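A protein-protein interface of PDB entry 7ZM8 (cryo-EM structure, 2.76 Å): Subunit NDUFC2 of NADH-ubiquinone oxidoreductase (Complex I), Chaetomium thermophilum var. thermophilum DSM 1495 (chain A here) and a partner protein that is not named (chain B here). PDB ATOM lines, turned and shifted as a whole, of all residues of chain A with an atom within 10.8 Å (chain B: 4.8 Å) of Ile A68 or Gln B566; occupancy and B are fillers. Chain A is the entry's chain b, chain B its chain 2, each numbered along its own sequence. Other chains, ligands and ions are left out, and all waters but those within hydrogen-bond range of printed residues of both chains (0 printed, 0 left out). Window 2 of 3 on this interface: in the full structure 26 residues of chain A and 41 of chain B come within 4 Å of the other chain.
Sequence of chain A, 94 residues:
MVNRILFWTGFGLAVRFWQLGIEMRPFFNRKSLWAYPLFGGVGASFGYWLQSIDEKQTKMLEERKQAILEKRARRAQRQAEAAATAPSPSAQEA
Ile B563 touches Gln A57 (CD1 to CG, 3.7 Å).
Ile B563 touches Met A60 (CG2 to SD, 3.5 Å).
Thr B562 touches Leu A61.
Ile B563 touches Leu A61 (CG1 to CD2, 3.6 Å).
Arg A64 touches Ser B570.
Ile A68 touches Gln B566 (CD1 to OE1, 3.9 Å).
Hydrophobic or aromatic side chains of chain A within 4 Å of the printed part of chain B: Met A60, Leu A61 and Ile A68.
Of the 11 printed residues of chain B, 4 touch a printed residue of chain A.
Hydrophobic or aromatic side chains of chain B that line the printed part of chain A: Ile B563.
Among the printed residues, 7 pairs touch across the chains.
Among the printed residues, no Asp or Glu carboxylate lies within 4 Å of a Lys or Arg side-chain nitrogen of the other chain.
The backbone carbonyl oxygen (O) of Leu A61 lies within hydrogen-bond range of the side-chain amino group (NZ) of Lys A65 (3.1 Å).
OE1 of Gln B364 is in hydrogen-bond range of OG1 of Thr B562, at 3.4 Å.
The backbone carbonyl oxygen (O) of Ile B567 is in hydrogen-bond range of the side-chain hydroxyl (OG) of Ser B570.
The guanidinium group (NE) of Arg A64 sits at hydrogen-bond distance from the side-chain amide oxygen (OE1) of Gln B566, at 2.9 Å.
Ile A68 touches just one residue of chain B: Gln B566 (3.9 Å).
Gln B566 touches two residues of chain A.
Ser B570 touches just one residue of chain A: Arg A64 (3.5 Å).
Of the printed residues of chain B, Met A60 touches Ile B563 (3.5 Å).
Of the printed residues of chain B, Arg A64 touches Gln B566 (2.9 Å) and Ser B570 (3.5 Å).
Printed residues of chain B within 4 Å of Leu A61: Thr B562 (3.8 Å) and Ile B563 (3.6 Å).
Printed residues of chain B within 4 Å of Gln A57: Ile B563 (3.7 Å).
Of the printed residues of chain A, Ile B563 touches Gln A57, Met A60 and Leu A61.
The nearest printed residue of chain B that does not touch Ile A68 is Ile B360 (6.8 Å).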
ATOM      1  N   GLN A  57     -29.382 -19.067 -30.948  1.00  0.00           N
ATOM      2  CA  GLN A  57     -28.535 -18.884 -29.775  1.00  0.00           C
ATOM      3  C   GLN A  57     -27.193 -19.572 -29.958  1.00  0.00           C
ATOM      4  O   GLN A  57     -26.159 -19.059 -29.516  1.00  0.00           O
ATOM      5  CB  GLN A  57     -29.227 -19.430 -28.532  1.00  0.00           C
ATOM      6  CG  GLN A  57     -30.309 -18.550 -27.969  1.00  0.00           C
ATOM      7  CD  GLN A  57     -31.135 -19.267 -26.938  1.00  0.00           C
ATOM      8  OE1 GLN A  57     -31.092 -20.489 -26.840  1.00  0.00           O
ATOM      9  NE2 GLN A  57     -31.891 -18.516 -26.161  1.00  0.00           N
ATOM     10  N   MET A  60     -24.893 -17.412 -32.118  1.00  0.00           N
ATOM     11  CA  MET A  60     -24.395 -16.188 -31.507  1.00  0.00           C
ATOM     12  C   MET A  60     -23.475 -16.477 -30.327  1.00  0.00           C
ATOM     13  O   MET A  60     -22.532 -15.720 -30.079  1.00  0.00           O
ATOM     14  CB  MET A  60     -25.565 -15.298 -31.097  1.00  0.00           C
ATOM     15  CG  MET A  60     -25.161 -13.850 -30.923  1.00  0.00           C
ATOM     16  SD  MET A  60     -26.197 -12.953 -29.773  1.00  0.00           S
ATOM     17  CE  MET A  60     -27.634 -12.746 -30.814  1.00  0.00           C
ATOM     18  N   LEU A  61     -23.725 -17.553 -29.585  1.00  0.00           N
ATOM     19  CA  LEU A  61     -22.775 -17.928 -28.547  1.00  0.00           C
ATOM     20  C   LEU A  61     -21.479 -18.447 -29.146  1.00  0.00           C
ATOM     21  O   LEU A  61     -20.414 -18.282 -28.545  1.00  0.00           O
ATOM     22  CB  LEU A  61     -23.385 -18.971 -27.612  1.00  0.00           C
ATOM     23  CG  LEU A  61     -24.327 -18.420 -26.544  1.00  0.00           C
ATOM     24  CD1 LEU A  61     -25.015 -19.545 -25.808  1.00  0.00           C
ATOM     25  CD2 LEU A  61     -23.577 -17.523 -25.584  1.00  0.00           C
ATOM     26  N   GLU A  62     -21.545 -19.082 -30.316  1.00  0.00           N
ATOM     27  CA  GLU A  62     -20.326 -19.482 -31.008  1.00  0.00           C
ATOM     28  C   GLU A  62     -19.518 -18.271 -31.446  1.00  0.00           C
ATOM     29  O   GLU A  62     -18.292 -18.243 -31.289  1.00  0.00           O
ATOM     30  CB  GLU A  62     -20.667 -20.355 -32.213  1.00  0.00           C
ATOM     31  CG  GLU A  62     -20.798 -21.829 -31.888  1.00  0.00           C
ATOM     32  CD  GLU A  62     -19.487 -22.448 -31.448  1.00  0.00           C
ATOM     33  OE1 GLU A  62     -18.447 -22.134 -32.061  1.00  0.00           O
ATOM     34  OE2 GLU A  62     -19.498 -23.248 -30.488  1.00  0.00           O
ATOM     35  N   GLU A  63     -20.174 -17.277 -32.042  1.00  0.00           N
ATOM     36  CA  GLU A  63     -19.503 -16.019 -32.465  1.00  0.00           C
ATOM     37  C   GLU A  63     -18.798 -15.367 -31.282  1.00  0.00           C
ATOM     38  O   GLU A  63     -17.671 -14.923 -31.468  1.00  0.00           O
ATOM     39  CB  GLU A  63     -20.520 -15.044 -33.047  1.00  0.00           C
ATOM     40  CG  GLU A  63     -20.988 -15.411 -34.442  1.00  0.00           C
ATOM     41  CD  GLU A  63     -19.928 -15.326 -35.527  1.00  0.00           C
ATOM     42  OE1 GLU A  63     -19.100 -14.394 -35.478  1.00  0.00           O
ATOM     43  OE2 GLU A  63     -19.931 -16.197 -36.419  1.00  0.00           O
ATOM     44  N   ARG A  64     -19.477 -15.238 -30.142  1.00  0.00           N
ATOM     45  CA  ARG A  64     -18.916 -14.551 -28.956  1.00  0.00           C
ATOM     46  C   ARG A  64     -17.638 -15.255 -28.508  1.00  0.00           C
ATOM     47  O   ARG A  64     -16.686 -14.569 -28.154  1.00  0.00           O
ATOM     48  CB  ARG A  64     -19.951 -14.558 -27.831  1.00  0.00           C
ATOM     49  CG  ARG A  64     -19.506 -13.890 -26.540  1.00  0.00           C
ATOM     50  CD  ARG A  64     -19.025 -12.467 -26.714  1.00  0.00           C
ATOM     51  NE  ARG A  64     -18.856 -11.887 -25.394  1.00  0.00           N
ATOM     52  CZ  ARG A  64     -17.963 -10.967 -25.072  1.00  0.00           C
ATOM     53  NH1 ARG A  64     -17.118 -10.509 -25.977  1.00  0.00           N
ATOM     54  NH2 ARG A  64     -17.908 -10.521 -23.833  1.00  0.00           N
ATOM     55  N   LYS A  65     -17.635 -16.579 -28.516  1.00  0.00           N
ATOM     56  CA  LYS A  65     -16.445 -17.297 -28.039  1.00  0.00           C
ATOM     57  C   LYS A  65     -15.320 -17.037 -29.027  1.00  0.00           C
ATOM     58  O   LYS A  65     -14.171 -17.010 -28.613  1.00  0.00           O
ATOM     59  CB  LYS A  65     -16.779 -18.781 -27.906  1.00  0.00           C
ATOM     60  CG  LYS A  65     -17.674 -19.121 -26.725  1.00  0.00           C
ATOM     61  CD  LYS A  65     -17.843 -20.597 -26.538  1.00  0.00           C
ATOM     62  CE  LYS A  65     -18.682 -21.240 -27.618  1.00  0.00           C
ATOM     63  NZ  LYS A  65     -20.126 -21.084 -27.338  1.00  0.00           N
ATOM     64  N   GLN A  66     -15.670 -16.821 -30.287  1.00  0.00           N
ATOM     65  CA  GLN A  66     -14.655 -16.456 -31.266  1.00  0.00           C
ATOM     66  C   GLN A  66     -14.176 -15.027 -31.058  1.00  0.00           C
ATOM     67  O   GLN A  66     -12.990 -14.736 -31.232  1.00  0.00           O
ATOM     68  CB  GLN A  66     -15.201 -16.646 -32.674  1.00  0.00           C
ATOM     69  CG  GLN A  66     -15.013 -18.049 -33.202  1.00  0.00           C
ATOM     70  CD  GLN A  66     -13.602 -18.556 -32.998  1.00  0.00           C
ATOM     71  OE1 GLN A  66     -13.356 -19.418 -32.156  1.00  0.00           O
ATOM     72  NE2 GLN A  66     -12.663 -18.017 -33.767  1.00  0.00           N
ATOM     73  N   ALA A  67     -15.061 -14.128 -30.631  1.00  0.00           N
ATOM     74  CA  ALA A  67     -14.664 -12.731 -30.342  1.00  0.00           C
ATOM     75  C   ALA A  67     -13.720 -12.639 -29.136  1.00  0.00           C
ATOM     76  O   ALA A  67     -12.729 -11.911 -29.234  1.00  0.00           O
ATOM     77  CB  ALA A  67     -15.888 -11.899 -30.118  1.00  0.00           C
ATOM     78  N   ILE A  68     -14.023 -13.332 -28.038  1.00  0.00           N
ATOM     79  CA  ILE A  68     -13.199 -13.256 -26.802  1.00  0.00           C
ATOM     80  C   ILE A  68     -11.818 -13.794 -27.164  1.00  0.00           C
ATOM     81  O   ILE A  68     -10.842 -13.356 -26.556  1.00  0.00           O
ATOM     82  CB  ILE A  68     -13.868 -13.999 -25.624  1.00  0.00           C
ATOM     83  CG1 ILE A  68     -15.335 -13.609 -25.451  1.00  0.00           C
ATOM     84  CG2 ILE A  68     -13.092 -13.810 -24.332  1.00  0.00           C
ATOM     85  CD1 ILE A  68     -16.121 -14.568 -24.589  1.00  0.00           C
ATOM     86  N   LEU A  69     -11.740 -14.656 -28.170  1.00  0.00           N
ATOM     87  CA  LEU A  69     -10.448 -15.271 -28.573  1.00  0.00           C
ATOM     88  C   LEU A  69      -9.678 -14.339 -29.508  1.00  0.00           C
ATOM     89  O   LEU A  69      -8.453 -14.401 -29.470  1.00  0.00           O
ATOM     90  CB  LEU A  69     -10.704 -16.657 -29.177  1.00  0.00           C
ATOM     91  CG  LEU A  69     -11.004 -17.757 -28.166  1.00  0.00           C
ATOM     92  CD1 LEU A  69     -11.381 -19.047 -28.871  1.00  0.00           C
ATOM     93  CD2 LEU A  69      -9.816 -17.979 -27.248  1.00  0.00           C
ATOM     94  N   GLU A  70     -10.356 -13.548 -30.344  1.00  0.00           N
ATOM     95  CA  GLU A  70      -9.643 -12.520 -31.099  1.00  0.00           C
ATOM     96  C   GLU A  70      -9.171 -11.394 -30.194  1.00  0.00           C
ATOM     97  O   GLU A  70      -8.061 -10.883 -30.360  1.00  0.00           O
ATOM     98  CB  GLU A  70     -10.513 -11.965 -32.227  1.00  0.00           C
ATOM     99  CG  GLU A  70     -11.322 -12.990 -33.001  1.00  0.00           C
ATOM    100  CD  GLU A  70     -10.473 -14.022 -33.739  1.00  0.00           C
ATOM    101  OE1 GLU A  70      -9.227 -13.947 -33.700  1.00  0.00           O
ATOM    102  OE2 GLU A  70     -11.066 -14.924 -34.367  1.00  0.00           O
ATOM    103  N   LYS A  71      -9.988 -11.001 -29.223  1.00  0.00           N
ATOM    104  CA  LYS A  71      -9.555  -9.929 -28.293  1.00  0.00           C
ATOM    105  C   LYS A  71      -8.318 -10.386 -27.521  1.00  0.00           C
ATOM    106  O   LYS A  71      -7.349  -9.618 -27.478  1.00  0.00           O
ATOM    107  CB  LYS A  71     -10.696  -9.540 -27.351  1.00  0.00           C
ATOM    108  CG  LYS A  71     -10.412  -8.349 -26.446  1.00  0.00           C
ATOM    109  CD  LYS A  71     -11.641  -7.841 -25.726  1.00  0.00           C
ATOM    110  CE  LYS A  71     -11.329  -6.714 -24.765  1.00  0.00           C
ATOM    111  NZ  LYS A  71     -10.519  -5.657 -25.414  1.00  0.00           N
ATOM    112  N   ARG A  72      -8.354 -11.579 -26.933  1.00  0.00           N
ATOM    113  CA  ARG A  72      -7.231 -12.086 -26.109  1.00  0.00           C
ATOM    114  C   ARG A  72      -5.992 -12.233 -26.985  1.00  0.00           C
ATOM    115  O   ARG A  72      -4.884 -12.187 -26.433  1.00  0.00           O
ATOM    116  CB  ARG A  72      -7.602 -13.434 -25.490  1.00  0.00           C
ATOM    117  CG  ARG A  72      -8.633 -13.349 -24.376  1.00  0.00           C
ATOM    118  CD  ARG A  72      -8.740 -14.681 -23.666  1.00  0.00           C
ATOM    119  NE  ARG A  72      -7.404 -15.139 -23.326  1.00  0.00           N
ATOM    120  CZ  ARG A  72      -6.747 -14.788 -22.229  1.00  0.00           C
ATOM    121  NH1 ARG A  72      -7.311 -13.980 -21.348  1.00  0.00           N
ATOM    122  NH2 ARG A  72      -5.533 -15.256 -22.009  1.00  0.00           N
ATOM    123  N   ALA A  73      -6.175 -12.401 -28.293  1.00  0.00           N
ATOM    124  CA  ALA A  73      -5.044 -12.632 -29.213  1.00  0.00           C
ATOM    125  C   ALA A  73      -4.522 -11.294 -29.724  1.00  0.00           C
ATOM    126  O   ALA A  73      -3.304 -11.115 -29.712  1.00  0.00           O
ATOM    127  CB  ALA A  73      -5.503 -13.504 -30.349  1.00  0.00           C
ATOM    128  N   ARG A  74      -5.402 -10.396 -30.166  1.00  0.00           N
ATOM    129  CA  ARG A  74      -4.941  -9.068 -30.556  1.00  0.00           C
ATOM    130  C   ARG A  74      -4.199  -8.388 -29.417  1.00  0.00           C
ATOM    131  O   ARG A  74      -3.182  -7.724 -29.640  1.00  0.00           O
ATOM    132  CB  ARG A  74      -6.123  -8.212 -31.008  1.00  0.00           C
ATOM    133  CG  ARG A  74      -6.539  -8.439 -32.447  1.00  0.00           C
ATOM    134  CD  ARG A  74      -7.679  -7.519 -32.840  1.00  0.00           C
ATOM    135  NE  ARG A  74      -8.930  -7.884 -32.180  1.00  0.00           N
ATOM    136  CZ  ARG A  74      -9.505  -7.165 -31.223  1.00  0.00           C
ATOM    137  NH1 ARG A  74      -8.942  -6.039 -30.811  1.00  0.00           N
ATOM    138  NH2 ARG A  74     -10.644  -7.570 -30.680  1.00  0.00           N
ATOM    139  N   ARG A  75      -4.705  -8.526 -28.190  1.00  0.00           N
ATOM    140  CA  ARG A  75      -4.008  -7.973 -27.037  1.00  0.00           C
ATOM    141  C   ARG A  75      -2.672  -8.665 -26.823  1.00  0.00           C
ATOM    142  O   ARG A  75      -1.670  -8.011 -26.514  1.00  0.00           O
ATOM    143  CB  ARG A  75      -4.883  -8.093 -25.790  1.00  0.00           C
ATOM    144  CG  ARG A  75      -4.264  -7.509 -24.539  1.00  0.00           C
ATOM    145  CD  ARG A  75      -4.983  -8.000 -23.293  1.00  0.00           C
ATOM    146  NE  ARG A  75      -6.398  -7.636 -23.295  1.00  0.00           N
ATOM    147  CZ  ARG A  75      -6.861  -6.421 -23.017  1.00  0.00           C
ATOM    148  NH1 ARG A  75      -6.023  -5.441 -22.709  1.00  0.00           N
ATOM    149  NH2 ARG A  75      -8.165  -6.185 -23.045  1.00  0.00           N
ATOM    150  N   ALA A  76      -2.634  -9.988 -26.980  1.00  0.00           N
ATOM    151  CA  ALA A  76      -1.378 -10.711 -26.826  1.00  0.00           C
ATOM    152  C   ALA A  76      -0.373 -10.299 -27.892  1.00  0.00           C
ATOM    153  O   ALA A  76       0.824 -10.175 -27.612  1.00  0.00           O
ATOM    154  CB  ALA A  76      -1.625 -12.217 -26.877  1.00  0.00           C
ATOM    155  N   ILE B 360     -19.665 -11.562 -14.536  1.00  0.00           N
ATOM    156  CA  ILE B 360     -20.467 -12.196 -15.615  1.00  0.00           C
ATOM    157  C   ILE B 360     -21.380 -13.264 -14.987  1.00  0.00           C
ATOM    158  O   ILE B 360     -22.592 -13.218 -15.256  1.00  0.00           O
ATOM    159  CB  ILE B 360     -19.536 -12.745 -16.721  1.00  0.00           C
ATOM    160  CG1 ILE B 360     -18.619 -11.649 -17.263  1.00  0.00           C
ATOM    161  CG2 ILE B 360     -20.329 -13.422 -17.824  1.00  0.00           C
ATOM    162  CD1 ILE B 360     -17.832 -12.051 -18.479  1.00  0.00           C
ATOM    163  N   GLN B 364     -25.743 -13.306 -14.707  1.00  0.00           N
ATOM    164  CA  GLN B 364     -26.572 -14.409 -15.265  1.00  0.00           C
ATOM    165  C   GLN B 364     -27.430 -15.013 -14.149  1.00  0.00           C
ATOM    166  O   GLN B 364     -28.606 -15.318 -14.412  1.00  0.00           O
ATOM    167  CB  GLN B 364     -25.681 -15.475 -15.900  1.00  0.00           C
ATOM    168  CG  GLN B 364     -24.937 -14.997 -17.133  1.00  0.00           C
ATOM    169  CD  GLN B 364     -23.788 -15.905 -17.485  1.00  0.00           C
ATOM    170  OE1 GLN B 364     -23.042 -15.654 -18.425  1.00  0.00           O
ATOM    171  NE2 GLN B 364     -23.633 -16.972 -16.718  1.00  0.00           N
ATOM    172  N   THR B 562     -27.139 -16.034 -20.654  1.00  0.00           N
ATOM    173  CA  THR B 562     -25.695 -16.009 -20.991  1.00  0.00           C
ATOM    174  C   THR B 562     -25.442 -14.992 -22.103  1.00  0.00           C
ATOM    175  O   THR B 562     -24.489 -14.240 -21.953  1.00  0.00           O
ATOM    176  CB  THR B 562     -25.054 -17.393 -21.177  1.00  0.00           C
ATOM    177  OG1 THR B 562     -23.657 -17.186 -21.382  1.00  0.00           O
ATOM    178  CG2 THR B 562     -25.580 -18.181 -22.351  1.00  0.00           C
ATOM    179  N   ILE B 563     -26.311 -14.929 -23.110  1.00  0.00           N
ATOM    180  CA  ILE B 563     -26.174 -13.940 -24.217  1.00  0.00           C
ATOM    181  C   ILE B 563     -26.448 -12.521 -23.705  1.00  0.00           C
ATOM    182  O   ILE B 563     -25.703 -11.616 -24.105  1.00  0.00           O
ATOM    183  CB  ILE B 563     -27.079 -14.323 -25.396  1.00  0.00           C
ATOM    184  CG1 ILE B 563     -26.686 -15.669 -26.003  1.00  0.00           C
ATOM    185  CG2 ILE B 563     -27.107 -13.227 -26.446  1.00  0.00           C
ATOM    186  CD1 ILE B 563     -27.622 -16.155 -27.076  1.00  0.00           C
ATOM    187  N   LEU B 564     -27.449 -12.315 -22.848  1.00  0.00           N
ATOM    188  CA  LEU B 564     -27.764 -10.922 -22.442  1.00  0.00           C
ATOM    189  C   LEU B 564     -26.580 -10.349 -21.671  1.00  0.00           C
ATOM    190  O   LEU B 564     -26.217  -9.193 -21.933  1.00  0.00           O
ATOM    191  CB  LEU B 564     -29.070 -10.851 -21.638  1.00  0.00           C
ATOM    192  CG  LEU B 564     -30.353 -11.159 -22.403  1.00  0.00           C
ATOM    193  CD1 LEU B 564     -31.545 -11.186 -21.462  1.00  0.00           C
ATOM    194  CD2 LEU B 564     -30.573 -10.153 -23.517  1.00  0.00           C
ATOM    195  N   VAL B 565     -26.005 -11.133 -20.765  1.00  0.00           N
ATOM    196  CA  VAL B 565     -24.841 -10.674 -19.955  1.00  0.00           C
ATOM    197  C   VAL B 565     -23.609 -10.530 -20.858  1.00  0.00           C
ATOM    198  O   VAL B 565     -22.782  -9.660 -20.575  1.00  0.00           O
ATOM    199  CB  VAL B 565     -24.635 -11.562 -18.717  1.00  0.00           C
ATOM    200  CG1 VAL B 565     -23.459 -11.096 -17.880  1.00  0.00           C
ATOM    201  CG2 VAL B 565     -25.900 -11.608 -17.878  1.00  0.00           C
ATOM    202  N   GLN B 566     -23.513 -11.293 -21.944  1.00  0.00           N
ATOM    203  CA  GLN B 566     -22.293 -11.216 -22.771  1.00  0.00           C
ATOM    204  C   GLN B 566     -22.320  -9.867 -23.473  1.00  0.00           C
ATOM    205  O   GLN B 566     -21.259  -9.303 -23.587  1.00  0.00           O
ATOM    206  CB  GLN B 566     -22.154 -12.393 -23.742  1.00  0.00           C
ATOM    207  CG  GLN B 566     -21.675 -13.700 -23.122  1.00  0.00           C
ATOM    208  CD  GLN B 566     -20.362 -13.635 -22.379  1.00  0.00           C
ATOM    209  OE1 GLN B 566     -19.333 -13.234 -22.909  1.00  0.00           O
ATOM    210  NE2 GLN B 566     -20.384 -14.073 -21.135  1.00  0.00           N
ATOM    211  N   ILE B 567     -23.478  -9.383 -23.912  1.00  0.00           N
ATOM    212  CA  ILE B 567     -23.621  -8.039 -24.543  1.00  0.00           C
ATOM    213  C   ILE B 567     -23.324  -6.929 -23.533  1.00  0.00           C
ATOM    214  O   ILE B 567     -22.612  -5.998 -23.882  1.00  0.00           O
ATOM    215  CB  ILE B 567     -25.002  -7.882 -25.214  1.00  0.00           C
ATOM    216  CG1 ILE B 567     -25.304  -9.027 -26.183  1.00  0.00           C
ATOM    217  CG2 ILE B 567     -25.145  -6.529 -25.885  1.00  0.00           C
ATOM    218  CD1 ILE B 567     -26.765  -9.147 -26.546  1.00  0.00           C
ATOM    219  N   LEU B 568     -23.826  -7.045 -22.313  1.00  0.00           N
ATOM    220  CA  LEU B 568     -23.632  -6.005 -21.272  1.00  0.00           C
ATOM    221  C   LEU B 568     -22.155  -5.867 -20.913  1.00  0.00           C
ATOM    222  O   LEU B 568     -21.718  -4.740 -20.753  1.00  0.00           O
ATOM    223  CB  LEU B 568     -24.448  -6.420 -20.044  1.00  0.00           C
ATOM    224  CG  LEU B 568     -24.161  -5.644 -18.760  1.00  0.00           C
ATOM    225  CD1 LEU B 568     -24.549  -4.183 -18.903  1.00  0.00           C
ATOM    226  CD2 LEU B 568     -24.878  -6.274 -17.581  1.00  0.00           C
ATOM    227  N   PHE B 569     -21.437  -6.975 -20.777  1.00  0.00           N
ATOM    228  CA  PHE B 569     -20.010  -6.959 -20.374  1.00  0.00           C
ATOM    229  C   PHE B 569     -19.134  -6.832 -21.614  1.00  0.00           C
ATOM    230  O   PHE B 569     -17.991  -6.402 -21.454  1.00  0.00           O
ATOM    231  CB  PHE B 569     -19.702  -8.234 -19.590  1.00  0.00           C
ATOM    232  CG  PHE B 569     -19.972  -8.161 -18.109  1.00  0.00           C
ATOM    233  CD1 PHE B 569     -21.266  -8.185 -17.618  1.00  0.00           C
ATOM    234  CD2 PHE B 569     -18.931  -8.086 -17.201  1.00  0.00           C
ATOM    235  CE1 PHE B 569     -21.514  -8.119 -16.259  1.00  0.00           C
ATOM    236  CE2 PHE B 569     -19.179  -8.023 -15.840  1.00  0.00           C
ATOM    237  CZ  PHE B 569     -20.469  -8.036 -15.373  1.00  0.00           C
ATOM    238  N   SER B 570     -19.689  -7.093 -22.799  1.00  0.00           N
ATOM    239  CA  SER B 570     -18.909  -7.143 -24.061  1.00  0.00           C
ATOM    240  C   SER B 570     -18.102  -5.879 -24.295  1.00  0.00           C
ATOM    241  O   SER B 570     -18.583  -4.800 -23.905  1.00  0.00           O
ATOM    242  CB  SER B 570     -19.779  -7.358 -25.232  1.00  0.00           C
ATOM    243  OG  SER B 570     -20.549  -6.198 -25.497  1.00  0.00           O
